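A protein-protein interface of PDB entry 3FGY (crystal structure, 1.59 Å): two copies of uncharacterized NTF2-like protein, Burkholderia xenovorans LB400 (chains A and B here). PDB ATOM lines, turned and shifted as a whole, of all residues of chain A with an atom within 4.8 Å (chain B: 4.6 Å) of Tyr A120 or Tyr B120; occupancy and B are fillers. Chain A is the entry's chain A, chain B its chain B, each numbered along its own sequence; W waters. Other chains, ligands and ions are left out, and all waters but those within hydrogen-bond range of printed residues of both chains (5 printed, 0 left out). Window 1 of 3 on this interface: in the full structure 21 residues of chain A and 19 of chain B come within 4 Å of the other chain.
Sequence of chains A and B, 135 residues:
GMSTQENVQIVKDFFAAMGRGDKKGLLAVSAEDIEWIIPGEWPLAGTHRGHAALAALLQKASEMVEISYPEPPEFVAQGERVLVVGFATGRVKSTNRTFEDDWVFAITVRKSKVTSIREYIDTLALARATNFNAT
Water W1 lies within hydrogen-bond range of the side-chain hydroxyl of Tyr B120 (2.6 Å) and the side-chain carboxylate of Asp A102 (2.8 Å).
Water W5 lies within hydrogen-bond range of the side-chain carboxylate of Asp B102 (2.6 Å) and the guanidinium group of Arg A118 (3.0 Å).
Water W2 lies within hydrogen-bond range of OD1 of Asp B102 (2.7 Å) and OH of Tyr A120 (2.7 Å).
Water W4 bridges the backbone carbonyl oxygen (O) of Ile B121 (2.9 Å) and the backbone carbonyl oxygen (O) of Ile A121 (3.2 Å).
Water W3 lies within hydrogen-bond range of the backbone carbonyl oxygen (O) of Ile A121 (2.9 Å) and the backbone carbonyl oxygen (O) of Ile B121 (3.2 Å).
N of Tyr A120 sits at hydrogen-bond distance from O of Val A104.
The backbone NH (N) of Ala A106 sits at hydrogen-bond distance from the backbone carbonyl oxygen (O) of Arg A118 (2.9 Å).
N of Tyr B120 lies within hydrogen-bond range of O of Val B104, at 2.8 Å.
N of Ala B106 is in hydrogen-bond range of O of Arg B118 (2.9 Å).
Printed residues of chain B within 4 Å of Val A104: Tyr B120 (3.6 Å).
Tyr A120 touches just these residues of chain B: Val B85, Asp B102, Trp B103, Val B104 and Tyr B120.
Printed residues of chain A within 4 Å of Val B104: Tyr A120 (3.6 Å).
Tyr B120 touches five residues of chain A.
The nearest printed residue of chain B that does not touch Tyr A120 is Ile B121 (5.1 Å).
The nearest printed residue of chain A that does not touch Tyr B120 is Ile A121 (5.2 Å).
The nearest printed residue of chain B that does not touch Ile A121 is Tyr B120 (5.2 Å).
The guanidinium group (NH1) of Arg B118 lies within salt-bridge range of the side-chain carboxylate (OD2) of Asp A102, at 3.4 Å.
The guanidinium group (NH2) of Arg A118 is in salt-bridge range of the side-chain carboxylate (OD2) of Asp B102.
O of Ile B121 lies close to O of Ile A121, 3.0 Å away.
Val A85 touches Tyr B120 (CG1 to OH, 3.3 Å).
Asp A102 touches Tyr B120 (O to CD2, 3.5 Å).
Trp A103 touches Tyr B120.
CG2 of Val A104 touches CD2 of Tyr B120 (3.6 Å).
OH of Tyr A120 touches CG1 of Val B85 (3.3 Å).
CD2 of Tyr A120 touches O of Asp B102, 3.5 Å away.
CE2 of Tyr A120 touches N of Trp B103, at 3.5 Å.
Tyr A120 touches Val B104 (CD1 to CG2, 3.6 Å).
Tyr A120 touches Tyr B120.
Val A85 touches Tyr B120, and with the chains exchanged Tyr A120 touches Val B85.
Asp A102 touches Arg B118, and with the chains exchanged Arg A118 touches Asp B102.
Asp A102 touches Tyr B120, and with the chains exchanged Tyr A120 touches Asp B102.
Ile A121 touches its own counterpart, Ile B121.
Positions printed for both chains: 85, 102, 103, 104, 106, 118, 119, 120 and 121.
Of the 12 pairs that touch across the chains among the printed residues, 12 have their exchanged pair printed and touching as well.
Of the 10 printed residues of chain A, 7 touch a printed residue of chain B.
Hydrophobic or aromatic side chains of chain A that line the printed part of chain B: Val A85, Val A104 and Tyr A120.
Of the 9 printed residues of chain B, 7 touch a printed residue of chain A.
Along chain B the printed residues that touch a printed residue of chain A span positions 85 to 121.
Among the printed residues, 12 pairs touch across the chains.
Among the printed residues, Asp or Glu carboxylates within 4 Å of a Lys or Arg side-chain nitrogen of the other chain: Asp A102 with Arg B118 and Arg A118 with Asp B102.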
ATOM      1  N   VAL A  85      -7.933 -21.767 -16.883  1.00  0.00           N
ATOM      2  CA  VAL A  85      -9.171 -22.373 -17.342  1.00  0.00           C
ATOM      3  C   VAL A  85      -9.378 -23.686 -16.599  1.00  0.00           C
ATOM      4  O   VAL A  85      -8.517 -24.548 -16.625  1.00  0.00           O
ATOM      5  CB  VAL A  85      -9.132 -22.654 -18.864  1.00  0.00           C
ATOM      6  CG1 VAL A  85     -10.486 -23.171 -19.348  1.00  0.00           C
ATOM      7  CG2 VAL A  85      -8.732 -21.340 -19.608  1.00  0.00           C
ATOM      8  N   ASP A 102     -17.744 -24.526 -14.648  1.00  0.00           N
ATOM      9  CA  ASP A 102     -16.663 -24.255 -15.618  1.00  0.00           C
ATOM     10  C   ASP A 102     -16.280 -22.796 -15.458  1.00  0.00           C
ATOM     11  O   ASP A 102     -17.129 -21.896 -15.531  1.00  0.00           O
ATOM     12  CB  ASP A 102     -17.074 -24.544 -17.052  1.00  0.00           C
ATOM     13  CG  ASP A 102     -16.950 -26.017 -17.380  1.00  0.00           C
ATOM     14  OD1 ASP A 102     -15.856 -26.461 -17.739  1.00  0.00           O
ATOM     15  OD2 ASP A 102     -17.959 -26.722 -17.247  1.00  0.00           O
ATOM     16  N   TRP A 103     -15.003 -22.548 -15.191  1.00  0.00           N
ATOM     17  CA  TRP A 103     -14.546 -21.223 -14.854  1.00  0.00           C
ATOM     18  C   TRP A 103     -13.272 -20.775 -15.582  1.00  0.00           C
ATOM     19  O   TRP A 103     -12.443 -21.594 -16.002  1.00  0.00           O
ATOM     20  CB  TRP A 103     -14.329 -21.108 -13.340  1.00  0.00           C
ATOM     21  CG  TRP A 103     -13.492 -22.204 -12.741  1.00  0.00           C
ATOM     22  CD1 TRP A 103     -13.934 -23.348 -12.122  1.00  0.00           C
ATOM     23  CD2 TRP A 103     -12.045 -22.257 -12.680  1.00  0.00           C
ATOM     24  NE1 TRP A 103     -12.858 -24.106 -11.694  1.00  0.00           N
ATOM     25  CE2 TRP A 103     -11.696 -23.453 -12.012  1.00  0.00           C
ATOM     26  CE3 TRP A 103     -11.023 -21.412 -13.119  1.00  0.00           C
ATOM     27  CZ2 TRP A 103     -10.360 -23.826 -11.771  1.00  0.00           C
ATOM     28  CZ3 TRP A 103      -9.676 -21.782 -12.859  1.00  0.00           C
ATOM     29  CH2 TRP A 103      -9.369 -22.981 -12.205  1.00  0.00           C
ATOM     30  N   VAL A 104     -13.115 -19.457 -15.677  1.00  0.00           N
ATOM     31  CA  VAL A 104     -11.852 -18.846 -16.059  1.00  0.00           C
ATOM     32  C   VAL A 104     -11.468 -17.794 -15.019  1.00  0.00           C
ATOM     33  O   VAL A 104     -12.282 -16.971 -14.605  1.00  0.00           O
ATOM     34  CB  VAL A 104     -11.946 -18.192 -17.458  1.00  0.00           C
ATOM     35  CG1 VAL A 104     -10.666 -17.354 -17.784  1.00  0.00           C
ATOM     36  CG2 VAL A 104     -12.217 -19.264 -18.535  1.00  0.00           C
ATOM     37  N   ALA A 106      -8.963 -14.716 -14.966  1.00  0.00           N
ATOM     38  CA  ALA A 106      -8.146 -13.867 -15.841  1.00  0.00           C
ATOM     39  C   ALA A 106      -7.278 -13.037 -14.921  1.00  0.00           C
ATOM     40  O   ALA A 106      -7.776 -12.222 -14.124  1.00  0.00           O
ATOM     41  CB  ALA A 106      -9.012 -12.970 -16.720  1.00  0.00           C
ATOM     42  N   ARG A 118      -9.931 -11.465 -12.277  1.00  0.00           N
ATOM     43  CA  ARG A 118     -11.361 -11.420 -12.507  1.00  0.00           C
ATOM     44  C   ARG A 118     -11.824 -12.846 -12.805  1.00  0.00           C
ATOM     45  O   ARG A 118     -11.263 -13.481 -13.684  1.00  0.00           O
ATOM     46  CB  ARG A 118     -11.674 -10.491 -13.678  1.00  0.00           C
ATOM     47  CG  ARG A 118     -13.085 -10.020 -13.658  1.00  0.00           C
ATOM     48  CD  ARG A 118     -13.573  -9.349 -14.926  1.00  0.00           C
ATOM     49  NE  ARG A 118     -15.013  -9.456 -14.806  1.00  0.00           N
ATOM     50  CZ  ARG A 118     -15.798  -8.568 -14.209  1.00  0.00           C
ATOM     51  NH1 ARG A 118     -15.338  -7.400 -13.849  1.00  0.00           N
ATOM     52  NH2 ARG A 118     -17.085  -8.847 -14.039  1.00  0.00           N
ATOM     53  N   GLU A 119     -12.832 -13.330 -12.074  1.00  0.00           N
ATOM     54  CA  GLU A 119     -13.425 -14.619 -12.342  1.00  0.00           C
ATOM     55  C   GLU A 119     -14.608 -14.529 -13.323  1.00  0.00           C
ATOM     56  O   GLU A 119     -15.433 -13.608 -13.260  1.00  0.00           O
ATOM     57  CB  GLU A 119     -13.943 -15.271 -11.057  1.00  0.00           C
ATOM     58  CG  GLU A 119     -12.966 -15.357  -9.923  1.00  0.00           C
ATOM     59  CD  GLU A 119     -13.480 -16.233  -8.774  1.00  0.00           C
ATOM     60  OE1 GLU A 119     -14.554 -16.902  -8.937  1.00  0.00           O
ATOM     61  OE2 GLU A 119     -12.820 -16.249  -7.719  1.00  0.00           O
ATOM     62  N   TYR A 120     -14.697 -15.562 -14.154  1.00  0.00           N
ATOM     63  CA  TYR A 120     -15.806 -15.785 -15.056  1.00  0.00           C
ATOM     64  C   TYR A 120     -16.334 -17.182 -14.682  1.00  0.00           C
ATOM     65  O   TYR A 120     -15.650 -18.172 -14.865  1.00  0.00           O
ATOM     66  CB  TYR A 120     -15.363 -15.712 -16.503  1.00  0.00           C
ATOM     67  CG  TYR A 120     -14.760 -14.373 -16.891  1.00  0.00           C
ATOM     68  CD1 TYR A 120     -13.438 -14.070 -16.553  1.00  0.00           C
ATOM     69  CD2 TYR A 120     -15.472 -13.420 -17.621  1.00  0.00           C
ATOM     70  CE1 TYR A 120     -12.858 -12.858 -16.928  1.00  0.00           C
ATOM     71  CE2 TYR A 120     -14.891 -12.214 -17.990  1.00  0.00           C
ATOM     72  CZ  TYR A 120     -13.601 -11.918 -17.643  1.00  0.00           C
ATOM     73  OH  TYR A 120     -12.985 -10.724 -18.021  1.00  0.00           O
ATOM     74  N   ILE A 121     -17.554 -17.215 -14.143  1.00  0.00           N
ATOM     75  CA  ILE A 121     -18.117 -18.390 -13.511  1.00  0.00           C
ATOM     76  C   ILE A 121     -19.602 -18.532 -13.869  1.00  0.00           C
ATOM     77  O   ILE A 121     -20.200 -17.645 -14.481  1.00  0.00           O
ATOM     78  CB  ILE A 121     -17.933 -18.316 -11.965  1.00  0.00           C
ATOM     79  CG1 ILE A 121     -18.723 -17.138 -11.394  1.00  0.00           C
ATOM     80  CG2 ILE A 121     -16.413 -18.284 -11.601  1.00  0.00           C
ATOM     81  CD1 ILE A 121     -18.552 -16.994  -9.914  1.00  0.00           C
ATOM     82  N   ASP A 122     -20.193 -19.666 -13.502  1.00  0.00           N
ATOM     83  CA  ASP A 122     -21.629 -19.887 -13.688  1.00  0.00           C
ATOM     84  C   ASP A 122     -22.389 -19.209 -12.556  1.00  0.00           C
ATOM     85  O   ASP A 122     -22.747 -19.823 -11.554  1.00  0.00           O
ATOM     86  CB  ASP A 122     -21.938 -21.390 -13.740  1.00  0.00           C
ATOM     87  CG  ASP A 122     -23.301 -21.700 -14.331  1.00  0.00           C
ATOM     88  OD1 ASP A 122     -24.200 -20.821 -14.310  1.00  0.00           O
ATOM     89  OD2 ASP A 122     -23.467 -22.858 -14.809  1.00  0.00           O
ATOM     90  N   VAL B  85     -11.520 -12.018 -24.461  1.00  0.00           N
ATOM     91  CA  VAL B  85     -12.029 -11.407 -23.216  1.00  0.00           C
ATOM     92  C   VAL B  85     -12.700 -10.120 -23.595  1.00  0.00           C
ATOM     93  O   VAL B  85     -12.079  -9.257 -24.216  1.00  0.00           O
ATOM     94  CB  VAL B  85     -10.870 -11.081 -22.226  1.00  0.00           C
ATOM     95  CG1 VAL B  85     -11.427 -10.579 -20.878  1.00  0.00           C
ATOM     96  CG2 VAL B  85      -9.961 -12.286 -22.072  1.00  0.00           C
ATOM     97  N   ASP B 102     -19.711  -9.393 -18.686  1.00  0.00           N
ATOM     98  CA  ASP B 102     -18.292  -9.612 -18.845  1.00  0.00           C
ATOM     99  C   ASP B 102     -18.084 -11.085 -19.183  1.00  0.00           C
ATOM    100  O   ASP B 102     -18.518 -12.007 -18.459  1.00  0.00           O
ATOM    101  CB  ASP B 102     -17.505  -9.253 -17.548  1.00  0.00           C
ATOM    102  CG  ASP B 102     -17.088  -7.782 -17.498  1.00  0.00           C
ATOM    103  OD1 ASP B 102     -16.172  -7.379 -18.252  1.00  0.00           O
ATOM    104  OD2 ASP B 102     -17.713  -7.016 -16.733  1.00  0.00           O
ATOM    105  N   TRP B 103     -17.422 -11.334 -20.305  1.00  0.00           N
ATOM    106  CA  TRP B 103     -17.326 -12.664 -20.843  1.00  0.00           C
ATOM    107  C   TRP B 103     -15.928 -13.062 -21.298  1.00  0.00           C
ATOM    108  O   TRP B 103     -15.085 -12.214 -21.637  1.00  0.00           O
ATOM    109  CB  TRP B 103     -18.303 -12.809 -22.043  1.00  0.00           C
ATOM    110  CG  TRP B 103     -18.217 -11.764 -23.067  1.00  0.00           C
ATOM    111  CD1 TRP B 103     -19.018 -10.675 -23.188  1.00  0.00           C
ATOM    112  CD2 TRP B 103     -17.310 -11.710 -24.190  1.00  0.00           C
ATOM    113  NE1 TRP B 103     -18.631  -9.914 -24.259  1.00  0.00           N
ATOM    114  CE2 TRP B 103     -17.600 -10.530 -24.907  1.00  0.00           C
ATOM    115  CE3 TRP B 103     -16.260 -12.504 -24.622  1.00  0.00           C
ATOM    116  CZ2 TRP B 103     -16.882 -10.144 -26.045  1.00  0.00           C
ATOM    117  CZ3 TRP B 103     -15.553 -12.123 -25.770  1.00  0.00           C
ATOM    118  CH2 TRP B 103     -15.863 -10.936 -26.449  1.00  0.00           C
ATOM    119  N   VAL B 104     -15.727 -14.368 -21.351  1.00  0.00           N
ATOM    120  CA  VAL B 104     -14.562 -14.959 -22.008  1.00  0.00           C
ATOM    121  C   VAL B 104     -15.057 -16.041 -22.959  1.00  0.00           C
ATOM    122  O   VAL B 104     -15.940 -16.827 -22.623  1.00  0.00           O
ATOM    123  CB  VAL B 104     -13.582 -15.629 -20.994  1.00  0.00           C
ATOM    124  CG1 VAL B 104     -12.454 -16.443 -21.734  1.00  0.00           C
ATOM    125  CG2 VAL B 104     -12.952 -14.599 -20.049  1.00  0.00           C
ATOM    126  N   ALA B 106     -13.405 -19.145 -24.867  1.00  0.00           N
ATOM    127  CA  ALA B 106     -12.187 -19.950 -24.959  1.00  0.00           C
ATOM    128  C   ALA B 106     -12.334 -20.796 -26.243  1.00  0.00           C
ATOM    129  O   ALA B 106     -13.284 -21.545 -26.375  1.00  0.00           O
ATOM    130  CB  ALA B 106     -11.974 -20.825 -23.752  1.00  0.00           C
ATOM    131  N   ARG B 118     -16.051 -22.514 -25.882  1.00  0.00           N
ATOM    132  CA  ARG B 118     -16.829 -22.505 -24.630  1.00  0.00           C
ATOM    133  C   ARG B 118     -16.898 -21.080 -24.145  1.00  0.00           C
ATOM    134  O   ARG B 118     -15.876 -20.397 -24.071  1.00  0.00           O
ATOM    135  CB  ARG B 118     -16.231 -23.370 -23.535  1.00  0.00           C
ATOM    136  CG  ARG B 118     -17.014 -23.258 -22.197  1.00  0.00           C
ATOM    137  CD  ARG B 118     -16.506 -24.212 -21.130  1.00  0.00           C
ATOM    138  NE  ARG B 118     -17.003 -25.563 -21.260  1.00  0.00           N
ATOM    139  CZ  ARG B 118     -18.161 -25.997 -20.755  1.00  0.00           C
ATOM    140  NH1 ARG B 118     -18.996 -25.174 -20.113  1.00  0.00           N
ATOM    141  NH2 ARG B 118     -18.495 -27.261 -20.908  1.00  0.00           N
ATOM    142  N   GLU B 119     -18.108 -20.638 -23.840  1.00  0.00           N
ATOM    143  CA  GLU B 119     -18.346 -19.325 -23.278  1.00  0.00           C
ATOM    144  C   GLU B 119     -18.412 -19.352 -21.758  1.00  0.00           C
ATOM    145  O   GLU B 119     -19.025 -20.262 -21.167  1.00  0.00           O
ATOM    146  CB  GLU B 119     -19.665 -18.717 -23.772  1.00  0.00           C
ATOM    147  CG  GLU B 119     -19.807 -18.623 -25.290  1.00  0.00           C
ATOM    148  CD  GLU B 119     -20.919 -17.756 -25.710  1.00  0.00           C
ATOM    149  OE1 GLU B 119     -21.491 -17.014 -24.869  1.00  0.00           O
ATOM    150  OE2 GLU B 119     -21.262 -17.819 -26.891  1.00  0.00           O
ATOM    151  N   TYR B 120     -17.824 -18.332 -21.136  1.00  0.00           N
ATOM    152  CA  TYR B 120     -17.866 -18.126 -19.700  1.00  0.00           C
ATOM    153  C   TYR B 120     -18.474 -16.753 -19.497  1.00  0.00           C
ATOM    154  O   TYR B 120     -17.889 -15.752 -19.918  1.00  0.00           O
ATOM    155  CB  TYR B 120     -16.463 -18.212 -19.101  1.00  0.00           C
ATOM    156  CG  TYR B 120     -15.738 -19.515 -19.384  1.00  0.00           C
ATOM    157  CD1 TYR B 120     -15.146 -19.739 -20.626  1.00  0.00           C
ATOM    158  CD2 TYR B 120     -15.612 -20.488 -18.405  1.00  0.00           C
ATOM    159  CE1 TYR B 120     -14.477 -20.923 -20.899  1.00  0.00           C
ATOM    160  CE2 TYR B 120     -14.947 -21.660 -18.647  1.00  0.00           C
ATOM    161  CZ  TYR B 120     -14.357 -21.884 -19.876  1.00  0.00           C
ATOM    162  OH  TYR B 120     -13.670 -23.073 -20.089  1.00  0.00           O
ATOM    163  N   ILE B 121     -19.690 -16.722 -18.961  1.00  0.00           N
ATOM    164  CA  ILE B 121     -20.533 -15.536 -19.037  1.00  0.00           C
ATOM    165  C   ILE B 121     -21.277 -15.354 -17.721  1.00  0.00           C
ATOM    166  O   ILE B 121     -21.303 -16.245 -16.841  1.00  0.00           O
ATOM    167  CB  ILE B 121     -21.544 -15.613 -20.222  1.00  0.00           C
ATOM    168  CG1 ILE B 121     -22.514 -16.767 -19.997  1.00  0.00           C
ATOM    169  CG2 ILE B 121     -20.798 -15.809 -21.545  1.00  0.00           C
ATOM    170  CD1 ILE B 121     -23.403 -17.088 -21.192  1.00  0.00           C
HETATM  171  O   HOH W   1     -13.656 -24.863 -18.179  1.00  0.00           O
HETATM  172  O   HOH W   2     -14.442  -8.984 -19.488  1.00  0.00           O
HETATM  173  O   HOH W   3     -19.302 -14.905 -14.802  1.00  0.00           O
HETATM  174  O   HOH W   4     -20.481 -18.977 -17.323  1.00  0.00           O
HETATM  175  O   HOH W   5     -19.605  -7.483 -14.971  1.00  0.00           O
